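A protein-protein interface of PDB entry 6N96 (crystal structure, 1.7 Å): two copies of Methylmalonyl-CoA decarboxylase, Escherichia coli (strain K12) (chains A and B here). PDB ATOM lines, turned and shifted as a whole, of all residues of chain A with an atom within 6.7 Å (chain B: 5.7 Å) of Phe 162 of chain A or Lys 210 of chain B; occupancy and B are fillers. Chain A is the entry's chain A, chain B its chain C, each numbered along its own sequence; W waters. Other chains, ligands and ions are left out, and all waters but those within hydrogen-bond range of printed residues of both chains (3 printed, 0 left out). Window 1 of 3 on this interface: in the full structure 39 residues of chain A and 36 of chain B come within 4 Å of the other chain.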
ATOM      1  N   MET A 131     -37.064   0.679   1.181  1.00  0.00           N
ATOM      2  CA  MET A 131     -35.729   0.250   1.659  1.00  0.00           C
ATOM      3  C   MET A 131     -35.109   1.460   2.368  1.00  0.00           C
ATOM      4  O   MET A 131     -34.905   2.473   1.717  1.00  0.00           O
ATOM      5  CB  MET A 131     -34.898  -0.253   0.465  1.00  0.00           C
ATOM      6  CG  MET A 131     -33.750  -1.142   0.822  1.00  0.00           C
ATOM      7  SD  MET A 131     -34.182  -2.587   1.822  1.00  0.00           S
ATOM      8  CE  MET A 131     -32.672  -2.845   2.740  1.00  0.00           C
ATOM      9  N   VAL A 134     -30.692   4.432   4.368  1.00  0.00           N
ATOM     10  CA  VAL A 134     -30.186   5.820   4.239  1.00  0.00           C
ATOM     11  C   VAL A 134     -30.999   6.744   5.142  1.00  0.00           C
ATOM     12  O   VAL A 134     -30.579   7.897   5.363  1.00  0.00           O
ATOM     13  CB  VAL A 134     -30.144   6.339   2.799  1.00  0.00           C
ATOM     14  CG1 VAL A 134     -29.347   5.411   1.927  1.00  0.00           C
ATOM     15  CG2 VAL A 134     -31.494   6.634   2.186  1.00  0.00           C
ATOM     16  N   PHE A 154     -30.342  -2.300 -11.788  1.00  0.00           N
ATOM     17  CA  PHE A 154     -29.511  -1.441 -10.912  1.00  0.00           C
ATOM     18  C   PHE A 154     -30.130  -0.050 -10.715  1.00  0.00           C
ATOM     19  O   PHE A 154     -30.146   0.452  -9.594  1.00  0.00           O
ATOM     20  CB  PHE A 154     -28.093  -1.326 -11.476  1.00  0.00           C
ATOM     21  CG  PHE A 154     -27.097  -2.182 -10.760  1.00  0.00           C
ATOM     22  CD1 PHE A 154     -27.405  -3.463 -10.366  1.00  0.00           C
ATOM     23  CD2 PHE A 154     -25.801  -1.734 -10.583  1.00  0.00           C
ATOM     24  CE1 PHE A 154     -26.446  -4.292  -9.793  1.00  0.00           C
ATOM     25  CE2 PHE A 154     -24.876  -2.526  -9.929  1.00  0.00           C
ATOM     26  CZ  PHE A 154     -25.195  -3.801  -9.549  1.00  0.00           C
ATOM     27  N   VAL A 157     -32.997  -0.260  -8.328  1.00  0.00           N
ATOM     28  CA  VAL A 157     -32.539  -0.582  -6.956  1.00  0.00           C
ATOM     29  C   VAL A 157     -31.909   0.657  -6.287  1.00  0.00           C
ATOM     30  O   VAL A 157     -32.186   0.941  -5.069  1.00  0.00           O
ATOM     31  CB  VAL A 157     -31.562  -1.761  -7.004  1.00  0.00           C
ATOM     32  CG1 VAL A 157     -30.918  -1.924  -5.639  1.00  0.00           C
ATOM     33  CG2 VAL A 157     -32.242  -3.049  -7.445  1.00  0.00           C
ATOM     34  N   LYS A 158     -31.099   1.409  -7.039  1.00  0.00           N
ATOM     35  CA  LYS A 158     -30.503   2.655  -6.544  1.00  0.00           C
ATOM     36  C   LYS A 158     -31.568   3.686  -6.206  1.00  0.00           C
ATOM     37  O   LYS A 158     -31.404   4.359  -5.194  1.00  0.00           O
ATOM     38  CB  LYS A 158     -29.435   3.188  -7.497  1.00  0.00           C
ATOM     39  CG  LYS A 158     -28.221   2.287  -7.542  1.00  0.00           C
ATOM     40  CD  LYS A 158     -27.305   2.733  -8.674  1.00  0.00           C
ATOM     41  CE  LYS A 158     -26.084   1.910  -8.799  1.00  0.00           C
ATOM     42  NZ  LYS A 158     -25.205   2.511  -9.821  1.00  0.00           N
ATOM     43  N   GLU A 159     -32.583   3.864  -7.042  1.00  0.00           N
ATOM     44  CA  GLU A 159     -33.688   4.772  -6.701  1.00  0.00           C
ATOM     45  C   GLU A 159     -34.278   4.348  -5.362  1.00  0.00           C
ATOM     46  O   GLU A 159     -34.463   5.222  -4.497  1.00  0.00           O
ATOM     47  CB  GLU A 159     -34.755   4.788  -7.799  1.00  0.00           C
ATOM     48  CG  GLU A 159     -35.947   5.655  -7.406  1.00  0.00           C
ATOM     49  CD  GLU A 159     -37.066   5.671  -8.413  1.00  0.00           C
ATOM     50  OE1 GLU A 159     -36.902   5.102  -9.502  1.00  0.00           O
ATOM     51  OE2 GLU A 159     -38.169   6.117  -8.032  1.00  0.00           O
ATOM     52  N   LEU A 160     -34.663   3.081  -5.231  1.00  0.00           N
ATOM     53  CA  LEU A 160     -35.309   2.595  -3.979  1.00  0.00           C
ATOM     54  C   LEU A 160     -34.411   2.912  -2.779  1.00  0.00           C
ATOM     55  O   LEU A 160     -34.877   3.434  -1.786  1.00  0.00           O
ATOM     56  CB  LEU A 160     -35.543   1.090  -4.074  1.00  0.00           C
ATOM     57  CG  LEU A 160     -36.676   0.644  -4.974  1.00  0.00           C
ATOM     58  CD1 LEU A 160     -36.726  -0.872  -5.033  1.00  0.00           C
ATOM     59  CD2 LEU A 160     -38.011   1.156  -4.451  1.00  0.00           C
ATOM     60  N   ILE A 161     -33.143   2.547  -2.852  1.00  0.00           N
ATOM     61  CA  ILE A 161     -32.239   2.712  -1.689  1.00  0.00           C
ATOM     62  C   ILE A 161     -31.924   4.197  -1.481  1.00  0.00           C
ATOM     63  O   ILE A 161     -31.937   4.634  -0.311  1.00  0.00           O
ATOM     64  CB  ILE A 161     -30.957   1.899  -1.841  1.00  0.00           C
ATOM     65  CG1 ILE A 161     -31.306   0.424  -1.926  1.00  0.00           C
ATOM     66  CG2 ILE A 161     -29.993   2.242  -0.709  1.00  0.00           C
ATOM     67  CD1 ILE A 161     -30.114  -0.449  -2.249  1.00  0.00           C
ATOM     68  N   PHE A 162     -31.601   4.968  -2.519  1.00  0.00           N
ATOM     69  CA  PHE A 162     -31.119   6.356  -2.280  1.00  0.00           C
ATOM     70  C   PHE A 162     -32.249   7.271  -1.824  1.00  0.00           C
ATOM     71  O   PHE A 162     -31.922   8.229  -1.132  1.00  0.00           O
ATOM     72  CB  PHE A 162     -30.393   6.905  -3.498  1.00  0.00           C
ATOM     73  CG  PHE A 162     -29.134   6.184  -3.893  1.00  0.00           C
ATOM     74  CD1 PHE A 162     -28.518   5.258  -3.072  1.00  0.00           C
ATOM     75  CD2 PHE A 162     -28.601   6.403  -5.155  1.00  0.00           C
ATOM     76  CE1 PHE A 162     -27.379   4.573  -3.468  1.00  0.00           C
ATOM     77  CE2 PHE A 162     -27.451   5.726  -5.547  1.00  0.00           C
ATOM     78  CZ  PHE A 162     -26.861   4.799  -4.710  1.00  0.00           C
ATOM     79  N   THR A 163     -33.495   7.036  -2.215  1.00  0.00           N
ATOM     80  CA  THR A 163     -34.647   7.892  -1.863  1.00  0.00           C
ATOM     81  C   THR A 163     -35.277   7.391  -0.583  1.00  0.00           C
ATOM     82  O   THR A 163     -35.904   8.185   0.108  1.00  0.00           O
ATOM     83  CB  THR A 163     -35.739   7.933  -2.938  1.00  0.00           C
ATOM     84  OG1 THR A 163     -36.348   6.654  -3.144  1.00  0.00           O
ATOM     85  CG2 THR A 163     -35.225   8.441  -4.260  1.00  0.00           C
ATOM     86  N   ALA A 164     -35.125   6.082  -0.299  1.00  0.00           N
ATOM     87  CA  ALA A 164     -35.899   5.402   0.749  1.00  0.00           C
ATOM     88  C   ALA A 164     -37.404   5.728   0.573  1.00  0.00           C
ATOM     89  O   ALA A 164     -38.113   5.675   1.584  1.00  0.00           O
ATOM     90  CB  ALA A 164     -35.416   5.816   2.108  1.00  0.00           C
ATOM     91  N   SER A 165     -37.878   6.069  -0.620  1.00  0.00           N
ATOM     92  CA  SER A 165     -39.330   6.373  -0.830  1.00  0.00           C
ATOM     93  C   SER A 165     -40.088   5.088  -1.048  1.00  0.00           C
ATOM     94  O   SER A 165     -39.601   4.195  -1.728  1.00  0.00           O
ATOM     95  CB  SER A 165     -39.548   7.282  -1.999  1.00  0.00           C
ATOM     96  OG  SER A 165     -38.888   8.502  -1.813  1.00  0.00           O
ATOM     97  N   ILE B  92     -17.861   8.356 -12.804  1.00  0.00           N
ATOM     98  CA  ILE B  92     -19.297   8.398 -12.387  1.00  0.00           C
ATOM     99  C   ILE B  92     -19.588   7.264 -11.400  1.00  0.00           C
ATOM    100  O   ILE B  92     -20.196   7.501 -10.349  1.00  0.00           O
ATOM    101  CB  ILE B  92     -20.176   8.321 -13.639  1.00  0.00           C
ATOM    102  CG1 ILE B  92     -20.109   9.653 -14.390  1.00  0.00           C
ATOM    103  CG2 ILE B  92     -21.601   7.922 -13.257  1.00  0.00           C
ATOM    104  CD1 ILE B  92     -20.808   9.622 -15.753  1.00  0.00           C
ATOM    105  N   GLN B  93     -19.097   6.065 -11.681  1.00  0.00           N
ATOM    106  CA  GLN B  93     -19.416   4.849 -10.898  1.00  0.00           C
ATOM    107  C   GLN B  93     -18.725   4.915  -9.528  1.00  0.00           C
ATOM    108  O   GLN B  93     -19.303   4.344  -8.586  1.00  0.00           O
ATOM    109  CB  GLN B  93     -19.027   3.609 -11.690  1.00  0.00           C
ATOM    110  CG  GLN B  93     -19.946   3.389 -12.873  1.00  0.00           C
ATOM    111  CD  GLN B  93     -19.509   2.224 -13.717  1.00  0.00           C
ATOM    112  OE1 GLN B  93     -18.312   1.953 -13.787  1.00  0.00           O
ATOM    113  NE2 GLN B  93     -20.474   1.558 -14.343  1.00  0.00           N
ATOM    114  N   LYS B  94     -17.552   5.537  -9.434  1.00  0.00           N
ATOM    115  CA  LYS B  94     -16.767   5.588  -8.162  1.00  0.00           C
ATOM    116  C   LYS B  94     -17.163   6.812  -7.333  1.00  0.00           C
ATOM    117  O   LYS B  94     -16.714   6.888  -6.172  1.00  0.00           O
ATOM    118  CB  LYS B  94     -15.273   5.575  -8.463  1.00  0.00           C
ATOM    119  CG  LYS B  94     -14.782   4.210  -8.924  1.00  0.00           C
ATOM    120  CD  LYS B  94     -13.326   4.168  -9.303  1.00  0.00           C
ATOM    121  CE  LYS B  94     -12.991   2.843  -9.961  1.00  0.00           C
ATOM    122  NZ  LYS B  94     -11.566   2.799 -10.367  1.00  0.00           N
ATOM    123  N   PHE B  95     -17.943   7.732  -7.902  1.00  0.00           N
ATOM    124  CA  PHE B  95     -18.279   9.024  -7.295  1.00  0.00           C
ATOM    125  C   PHE B  95     -19.136   8.777  -6.079  1.00  0.00           C
ATOM    126  O   PHE B  95     -20.114   8.054  -6.168  1.00  0.00           O
ATOM    127  CB  PHE B  95     -18.968   9.956  -8.292  1.00  0.00           C
ATOM    128  CG  PHE B  95     -18.889  11.408  -7.918  1.00  0.00           C
ATOM    129  CD1 PHE B  95     -17.666  12.062  -7.975  1.00  0.00           C
ATOM    130  CD2 PHE B  95     -19.988  12.084  -7.441  1.00  0.00           C
ATOM    131  CE1 PHE B  95     -17.579  13.398  -7.637  1.00  0.00           C
ATOM    132  CE2 PHE B  95     -19.895  13.429  -7.092  1.00  0.00           C
ATOM    133  CZ  PHE B  95     -18.671  14.055  -7.137  1.00  0.00           C
ATOM    134  N   PRO B  96     -18.770   9.306  -4.891  1.00  0.00           N
ATOM    135  CA  PRO B  96     -19.478   8.936  -3.687  1.00  0.00           C
ATOM    136  C   PRO B  96     -20.857   9.570  -3.504  1.00  0.00           C
ATOM    137  O   PRO B  96     -21.398   9.480  -2.413  1.00  0.00           O
ATOM    138  CB  PRO B  96     -18.518   9.359  -2.557  1.00  0.00           C
ATOM    139  CG  PRO B  96     -17.740  10.501  -3.155  1.00  0.00           C
ATOM    140  CD  PRO B  96     -17.557  10.097  -4.619  1.00  0.00           C
ATOM    141  N   LYS B  97     -21.376  10.274  -4.484  1.00  0.00           N
ATOM    142  CA  LYS B  97     -22.709  10.883  -4.400  1.00  0.00           C
ATOM    143  C   LYS B  97     -23.517  10.274  -5.534  1.00  0.00           C
ATOM    144  O   LYS B  97     -22.956   9.910  -6.560  1.00  0.00           O
ATOM    145  CB  LYS B  97     -22.595  12.405  -4.485  1.00  0.00           C
ATOM    146  CG  LYS B  97     -21.715  12.999  -3.361  1.00  0.00           C
ATOM    147  CD  LYS B  97     -21.305  14.348  -3.602  1.00  0.00           C
ATOM    148  CE  LYS B  97     -20.172  14.842  -2.728  1.00  0.00           C
ATOM    149  NZ  LYS B  97     -20.332  14.614  -1.271  1.00  0.00           N
ATOM    150  N   PRO B  98     -24.843  10.232  -5.428  1.00  0.00           N
ATOM    151  CA  PRO B  98     -25.670   9.838  -6.543  1.00  0.00           C
ATOM    152  C   PRO B  98     -25.534  10.850  -7.674  1.00  0.00           C
ATOM    153  O   PRO B  98     -25.437  12.051  -7.445  1.00  0.00           O
ATOM    154  CB  PRO B  98     -27.118   9.827  -6.021  1.00  0.00           C
ATOM    155  CG  PRO B  98     -26.889   9.673  -4.535  1.00  0.00           C
ATOM    156  CD  PRO B  98     -25.676  10.546  -4.256  1.00  0.00           C
ATOM    157  N   ILE B  99     -25.552  10.298  -8.880  1.00  0.00           N
ATOM    158  CA  ILE B  99     -25.500  11.071 -10.134  1.00  0.00           C
ATOM    159  C   ILE B  99     -26.724  10.660 -10.918  1.00  0.00           C
ATOM    160  O   ILE B  99     -26.875   9.482 -11.284  1.00  0.00           O
ATOM    161  CB  ILE B  99     -24.202  10.843 -10.883  1.00  0.00           C
ATOM    162  CG1 ILE B  99     -23.005  11.266 -10.025  1.00  0.00           C
ATOM    163  CG2 ILE B  99     -24.231  11.533 -12.231  1.00  0.00           C
ATOM    164  CD1 ILE B  99     -21.678  10.983 -10.654  1.00  0.00           C
ATOM    165  N   ASP B 119     -26.470   6.694 -11.781  1.00  0.00           N
ATOM    166  CA  ASP B 119     -27.263   5.998 -10.742  1.00  0.00           C
ATOM    167  C   ASP B 119     -28.747   5.894 -11.100  1.00  0.00           C
ATOM    168  O   ASP B 119     -29.385   4.866 -10.778  1.00  0.00           O
ATOM    169  CB  ASP B 119     -27.018   6.624  -9.375  1.00  0.00           C
ATOM    170  CG  ASP B 119     -25.521   6.502  -9.051  1.00  0.00           C
ATOM    171  OD1 ASP B 119     -24.950   5.360  -9.207  1.00  0.00           O
ATOM    172  OD2 ASP B 119     -24.897   7.557  -8.822  1.00  0.00           O
ATOM    173  N   LEU B 120     -29.321   6.953 -11.647  1.00  0.00           N
ATOM    174  CA  LEU B 120     -30.758   7.041 -11.987  1.00  0.00           C
ATOM    175  C   LEU B 120     -30.863   7.823 -13.286  1.00  0.00           C
ATOM    176  O   LEU B 120     -29.970   8.676 -13.580  1.00  0.00           O
ATOM    177  CB  LEU B 120     -31.502   7.838 -10.915  1.00  0.00           C
ATOM    178  CG  LEU B 120     -31.912   7.177  -9.612  1.00  0.00           C
ATOM    179  CD1 LEU B 120     -30.798   7.254  -8.625  1.00  0.00           C
ATOM    180  CD2 LEU B 120     -33.125   7.927  -9.067  1.00  0.00           C
ATOM    181  N   HIS B 197     -34.759  15.392  -2.145  1.00  0.00           N
ATOM    182  CA  HIS B 197     -35.198  14.303  -1.222  1.00  0.00           C
ATOM    183  C   HIS B 197     -33.981  13.441  -0.856  1.00  0.00           C
ATOM    184  O   HIS B 197     -33.702  13.238   0.334  1.00  0.00           O
ATOM    185  CB  HIS B 197     -36.344  13.487  -1.827  1.00  0.00           C
ATOM    186  CG  HIS B 197     -36.971  12.595  -0.826  1.00  0.00           C
ATOM    187  ND1 HIS B 197     -36.950  11.225  -0.940  1.00  0.00           N
ATOM    188  CD2 HIS B 197     -37.509  12.856   0.371  1.00  0.00           C
ATOM    189  CE1 HIS B 197     -37.537  10.682   0.110  1.00  0.00           C
ATOM    190  NE2 HIS B 197     -37.867  11.638   0.942  1.00  0.00           N
ATOM    191  N   ILE B 198     -33.212  13.017  -1.857  1.00  0.00           N
ATOM    192  CA  ILE B 198     -31.968  12.213  -1.654  1.00  0.00           C
ATOM    193  C   ILE B 198     -30.995  12.988  -0.775  1.00  0.00           C
ATOM    194  O   ILE B 198     -30.309  12.382   0.075  1.00  0.00           O
ATOM    195  CB  ILE B 198     -31.330  11.830  -2.995  1.00  0.00           C
ATOM    196  CG1 ILE B 198     -32.192  10.803  -3.721  1.00  0.00           C
ATOM    197  CG2 ILE B 198     -29.922  11.352  -2.772  1.00  0.00           C
ATOM    198  CD1 ILE B 198     -31.740  10.568  -5.134  1.00  0.00           C
ATOM    199  N   LYS B 201     -30.814  12.524   3.031  1.00  0.00           N
ATOM    200  CA  LYS B 201     -30.550  11.158   3.534  1.00  0.00           C
ATOM    201  C   LYS B 201     -29.098  11.078   3.961  1.00  0.00           C
ATOM    202  O   LYS B 201     -28.343  12.033   3.795  1.00  0.00           O
ATOM    203  CB  LYS B 201     -30.979  10.108   2.487  1.00  0.00           C
ATOM    204  CG  LYS B 201     -32.398  10.246   1.988  1.00  0.00           C
ATOM    205  CD  LYS B 201     -33.450  10.178   3.060  1.00  0.00           C
ATOM    206  CE  LYS B 201     -34.864  10.200   2.534  1.00  0.00           C
ATOM    207  NZ  LYS B 201     -35.827   9.998   3.628  1.00  0.00           N
ATOM    208  N   ALA B 205     -23.881   6.450   4.190  1.00  0.00           N
ATOM    209  CA  ALA B 205     -24.612   5.200   3.896  1.00  0.00           C
ATOM    210  C   ALA B 205     -24.828   5.122   2.375  1.00  0.00           C
ATOM    211  O   ALA B 205     -24.571   4.078   1.750  1.00  0.00           O
ATOM    212  CB  ALA B 205     -25.910   5.132   4.666  1.00  0.00           C
ATOM    213  N   ILE B 206     -25.228   6.240   1.747  1.00  0.00           N
ATOM    214  CA  ILE B 206     -25.415   6.240   0.270  1.00  0.00           C
ATOM    215  C   ILE B 206     -24.083   5.876  -0.392  1.00  0.00           C
ATOM    216  O   ILE B 206     -24.109   5.033  -1.291  1.00  0.00           O
ATOM    217  CB  ILE B 206     -25.931   7.591  -0.215  1.00  0.00           C
ATOM    218  CG1 ILE B 206     -27.388   7.761   0.186  1.00  0.00           C
ATOM    219  CG2 ILE B 206     -25.782   7.708  -1.725  1.00  0.00           C
ATOM    220  CD1 ILE B 206     -27.907   9.176  -0.015  1.00  0.00           C
ATOM    221  N   ALA B 207     -22.969   6.480   0.018  1.00  0.00           N
ATOM    222  CA  ALA B 207     -21.682   6.275  -0.669  1.00  0.00           C
ATOM    223  C   ALA B 207     -21.281   4.799  -0.536  1.00  0.00           C
ATOM    224  O   ALA B 207     -20.841   4.222  -1.528  1.00  0.00           O
ATOM    225  CB  ALA B 207     -20.607   7.222  -0.151  1.00  0.00           C
ATOM    226  N   VAL B 208     -21.368   4.196   0.644  1.00  0.00           N
ATOM    227  CA  VAL B 208     -20.865   2.797   0.792  1.00  0.00           C
ATOM    228  C   VAL B 208     -21.787   1.839   0.031  1.00  0.00           C
ATOM    229  O   VAL B 208     -21.280   0.913  -0.581  1.00  0.00           O
ATOM    230  CB  VAL B 208     -20.634   2.399   2.260  1.00  0.00           C
ATOM    231  CG1 VAL B 208     -21.924   2.170   2.986  1.00  0.00           C
ATOM    232  CG2 VAL B 208     -19.764   1.170   2.325  1.00  0.00           C
ATOM    233  N   ILE B 209     -23.104   2.071   0.016  1.00  0.00           N
ATOM    234  CA  ILE B 209     -24.055   1.175  -0.675  1.00  0.00           C
ATOM    235  C   ILE B 209     -23.807   1.325  -2.187  1.00  0.00           C
ATOM    236  O   ILE B 209     -23.827   0.292  -2.910  1.00  0.00           O
ATOM    237  CB  ILE B 209     -25.512   1.440  -0.260  1.00  0.00           C
ATOM    238  CG1 ILE B 209     -25.744   1.088   1.205  1.00  0.00           C
ATOM    239  CG2 ILE B 209     -26.464   0.708  -1.168  1.00  0.00           C
ATOM    240  CD1 ILE B 209     -27.053   1.557   1.733  1.00  0.00           C
ATOM    241  N   LYS B 210     -23.555   2.537  -2.672  1.00  0.00           N
ATOM    242  CA  LYS B 210     -23.227   2.717  -4.110  1.00  0.00           C
ATOM    243  C   LYS B 210     -21.974   1.909  -4.484  1.00  0.00           C
ATOM    244  O   LYS B 210     -21.935   1.288  -5.538  1.00  0.00           O
ATOM    245  CB  LYS B 210     -22.978   4.202  -4.397  1.00  0.00           C
ATOM    246  CG  LYS B 210     -22.715   4.466  -5.859  1.00  0.00           C
ATOM    247  CD  LYS B 210     -22.658   5.954  -6.268  1.00  0.00           C
ATOM    248  CE  LYS B 210     -21.956   6.097  -7.603  1.00  0.00           C
ATOM    249  NZ  LYS B 210     -22.196   7.448  -8.162  1.00  0.00           N
ATOM    250  N   GLU B 211     -20.933   1.970  -3.663  1.00  0.00           N
ATOM    251  CA  GLU B 211     -19.669   1.261  -3.901  1.00  0.00           C
ATOM    252  C   GLU B 211     -19.893  -0.248  -3.825  1.00  0.00           C
ATOM    253  O   GLU B 211     -19.323  -0.952  -4.657  1.00  0.00           O
ATOM    254  CB  GLU B 211     -18.609   1.702  -2.918  1.00  0.00           C
ATOM    255  CG  GLU B 211     -17.261   1.057  -3.158  1.00  0.00           C
ATOM    256  CD  GLU B 211     -16.546   1.376  -4.480  1.00  0.00           C
ATOM    257  OE1 GLU B 211     -17.044   2.171  -5.339  1.00  0.00           O
ATOM    258  OE2 GLU B 211     -15.437   0.821  -4.662  1.00  0.00           O
ATOM    259  N   GLU B 212     -20.755  -0.714  -2.924  1.00  0.00           N
ATOM    260  CA  GLU B 212     -21.091  -2.154  -2.824  1.00  0.00           C
ATOM    261  C   GLU B 212     -21.783  -2.600  -4.105  1.00  0.00           C
ATOM    262  O   GLU B 212     -21.381  -3.625  -4.669  1.00  0.00           O
ATOM    263  CB  GLU B 212     -21.963  -2.442  -1.618  1.00  0.00           C
ATOM    264  CG  GLU B 212     -21.193  -2.370  -0.319  1.00  0.00           C
ATOM    265  CD  GLU B 212     -22.103  -2.489   0.897  1.00  0.00           C
ATOM    266  OE1 GLU B 212     -23.288  -2.092   0.782  1.00  0.00           O
ATOM    267  OE2 GLU B 212     -21.647  -2.918   1.926  1.00  0.00           O
ATOM    268  N   LEU B 213     -22.721  -1.807  -4.621  1.00  0.00           N
ATOM    269  CA  LEU B 213     -23.380  -2.154  -5.906  1.00  0.00           C
ATOM    270  C   LEU B 213     -22.348  -2.140  -7.010  1.00  0.00           C
ATOM    271  O   LEU B 213     -22.432  -3.003  -7.891  1.00  0.00           O
ATOM    272  CB  LEU B 213     -24.524  -1.191  -6.183  1.00  0.00           C
ATOM    273  CG  LEU B 213     -25.762  -1.410  -5.325  1.00  0.00           C
ATOM    274  CD1 LEU B 213     -26.605  -0.140  -5.346  1.00  0.00           C
ATOM    275  CD2 LEU B 213     -26.546  -2.605  -5.836  1.00  0.00           C
ATOM    276  N   ARG B 214     -21.439  -1.179  -7.014  1.00  0.00           N
ATOM    277  CA  ARG B 214     -20.423  -1.087  -8.097  1.00  0.00           C
ATOM    278  C   ARG B 214     -19.610  -2.379  -8.104  1.00  0.00           C
ATOM    279  O   ARG B 214     -19.415  -2.988  -9.186  1.00  0.00           O
ATOM    280  CB  ARG B 214     -19.487   0.117  -7.948  1.00  0.00           C
ATOM    281  CG  ARG B 214     -18.576   0.304  -9.145  1.00  0.00           C
ATOM    282  CD  ARG B 214     -17.552   1.417  -8.952  1.00  0.00           C
ATOM    283  NE  ARG B 214     -16.539   1.042  -7.974  1.00  0.00           N
ATOM    284  CZ  ARG B 214     -15.495   0.271  -8.254  1.00  0.00           C
ATOM    285  NH1 ARG B 214     -15.276  -0.122  -9.497  1.00  0.00           N
ATOM    286  NH2 ARG B 214     -14.646  -0.060  -7.298  1.00  0.00           N
ATOM    287  N   VAL B 215     -19.084  -2.771  -6.957  1.00  0.00           N
ATOM    288  CA  VAL B 215     -18.220  -3.980  -6.849  1.00  0.00           C
ATOM    289  C   VAL B 215     -19.026  -5.233  -7.224  1.00  0.00           C
ATOM    290  O   VAL B 215     -18.478  -6.103  -7.974  1.00  0.00           O
ATOM    291  CB  VAL B 215     -17.595  -4.028  -5.445  1.00  0.00           C
ATOM    292  CG1 VAL B 215     -16.961  -5.371  -5.172  1.00  0.00           C
ATOM    293  CG2 VAL B 215     -16.580  -2.914  -5.285  1.00  0.00           C
HETATM  294  O   HOH W   1     -38.063   8.690   2.215  1.00  0.00           O
HETATM  295  O   HOH W   2     -22.949   4.653 -10.836  1.00  0.00           O
HETATM  296  O   HOH W   3     -23.422   1.364  -8.204  1.00  0.00           O
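Phe 162 of chain A touches just these residues of chain B: Pro 98, Asp 119, Ile 198, Lys 201, Ile 206 and Lys 210.
Of chain A, only Phe 162 comes within 4 Å of Lys 210 of chain B.
Of the printed residues of chain B, Ile 161 of chain A touches Ile 209.
Of the printed residues of chain A, Ile 206 of chain B touches Val 134 (3.5 Å) and Phe 162 (3.9 Å).
Printed residues of chain A within 4 Å of His 197 of chain B: Thr 163 and Ser 165.
Of the printed residues of chain A, Leu 213 of chain B touches Phe 154 (3.2 Å) and Lys 158 (3.7 Å).
Printed residues of chain B within 4 Å of Val 134 of chain A: Lys 201 (3.5 Å) and Ile 206 (3.5 Å).
Ala 205 of chain B touches none of the printed residues of chain A.
Ala 164 of chain A touches none of the printed residues of chain B.
The nearest residue of chain B that does not touch Phe 162 of chain A is Leu 120 of chain B (4.2 Å).
The nearest printed residue of chain A that does not touch Leu 213 of chain B is Val 157 of chain A (4.4 Å).
Water W3 lies within hydrogen-bond range of NZ of Lys 158 of chain A (2.7 Å), O of Lys 210 of chain B (3.1 Å) and N of Arg 214 of chain B (3.4 Å).
Water W2 lies within hydrogen-bond range of OD1 of Asp 119 of chain B (2.7 Å) and NZ of Lys 158 of chain A (3.3 Å).
Water W1 lies within hydrogen-bond range of NZ of Lys 201 of chain B (3.0 Å), O of Thr 163 of chain A (3.1 Å), O of Ala 164 of chain A (3.1 Å) and NE2 of His 197 of chain B (3.2 Å).
No position is printed for both chains.
Of the 24 printed residues of chain B, 10 touch a printed residue of chain A.
Hydrophobic or aromatic side chains of chain B within 4 Å of the printed part of chain A: Pro 98, Leu 120, His 197, Ile 198, Ile 206, Ile 209 and Leu 213.
Along chain B the printed residues that touch a printed residue of chain A span positions 98 to 213.
Hydrophobic or aromatic side chains of chain A that line the printed part of chain B: Val 134, Phe 154, Ile 161 and Phe 162.
Among the printed residues, Asp or Glu carboxylates within 4 Å of a Lys or Arg side-chain nitrogen of the other chain: Lys 158 of chain A with Asp 119 of chain B (2.9 Å).
The side-chain amino group (NZ) of Lys 158 of chain A lies within salt-bridge range of the side-chain carboxylate (OD1) of Asp 119 of chain B (2.9 Å).
A ring nitrogen (ND1) of His 197 of chain B lies close to the backbone carbonyl oxygen of Thr 163 of chain A, at 3.4 Å.
The side-chain hydroxyl (OG) of Ser 165 of chain A sits close to a ring nitrogen (ND1) of His 197 of chain B, at 3.5 Å.
OG1 of Thr 163 of chain A lies within hydrogen-bond range of O of Glu 159 of chain A.
NZ of Lys 210 of chain B sits at hydrogen-bond distance from O of Phe 95 of chain B (2.9 Å).
The backbone carbonyl oxygen (O) of Lys 97 of chain B sits at hydrogen-bond distance from the side-chain amino group (NZ) of Lys 210 of chain B, 3.0 Å away.
The backbone NH (N) of Ile 99 of chain B sits at hydrogen-bond distance from the side-chain carboxylate (OD2) of Asp 119 of chain B (2.8 Å).
The side-chain carboxylate of Asp 119 of chain B lies within salt-bridge range of the side-chain amino group of Lys 210 of chain B (2.8 Å).
Among the printed residues, merely in contact across the chains: Val 134 of chain A with Lys 201 of chain B (3.5 Å), Val 134 of chain A with Ile 206 of chain B (3.5 Å), Phe 154 of chain A with Leu 213 of chain B (3.2 Å), Lys 158 of chain A with Leu 213 of chain B (3.7 Å), Glu 159 of chain A with Leu 120 of chain B (3.8 Å), Ile 161 of chain A with Ile 209 of chain B (3.9 Å), Phe 162 of chain A with Pro 98 of chain B (3.7 Å), Phe 162 of chain A with Asp 119 of chain B (3.96 Å), Phe 162 of chain A with Ile 198 of chain B (3.7 Å), Phe 162 of chain A with Lys 201 of chain B (3.7 Å), Phe 162 of chain A with Ile 206 of chain B (3.9 Å), Phe 162 of chain A with Lys 210 of chain B (3.9 Å), Thr 163 of chain A with Ile 198 of chain B (3.9 Å) and Thr 163 of chain A with Lys 201 of chain B (3.3 Å).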
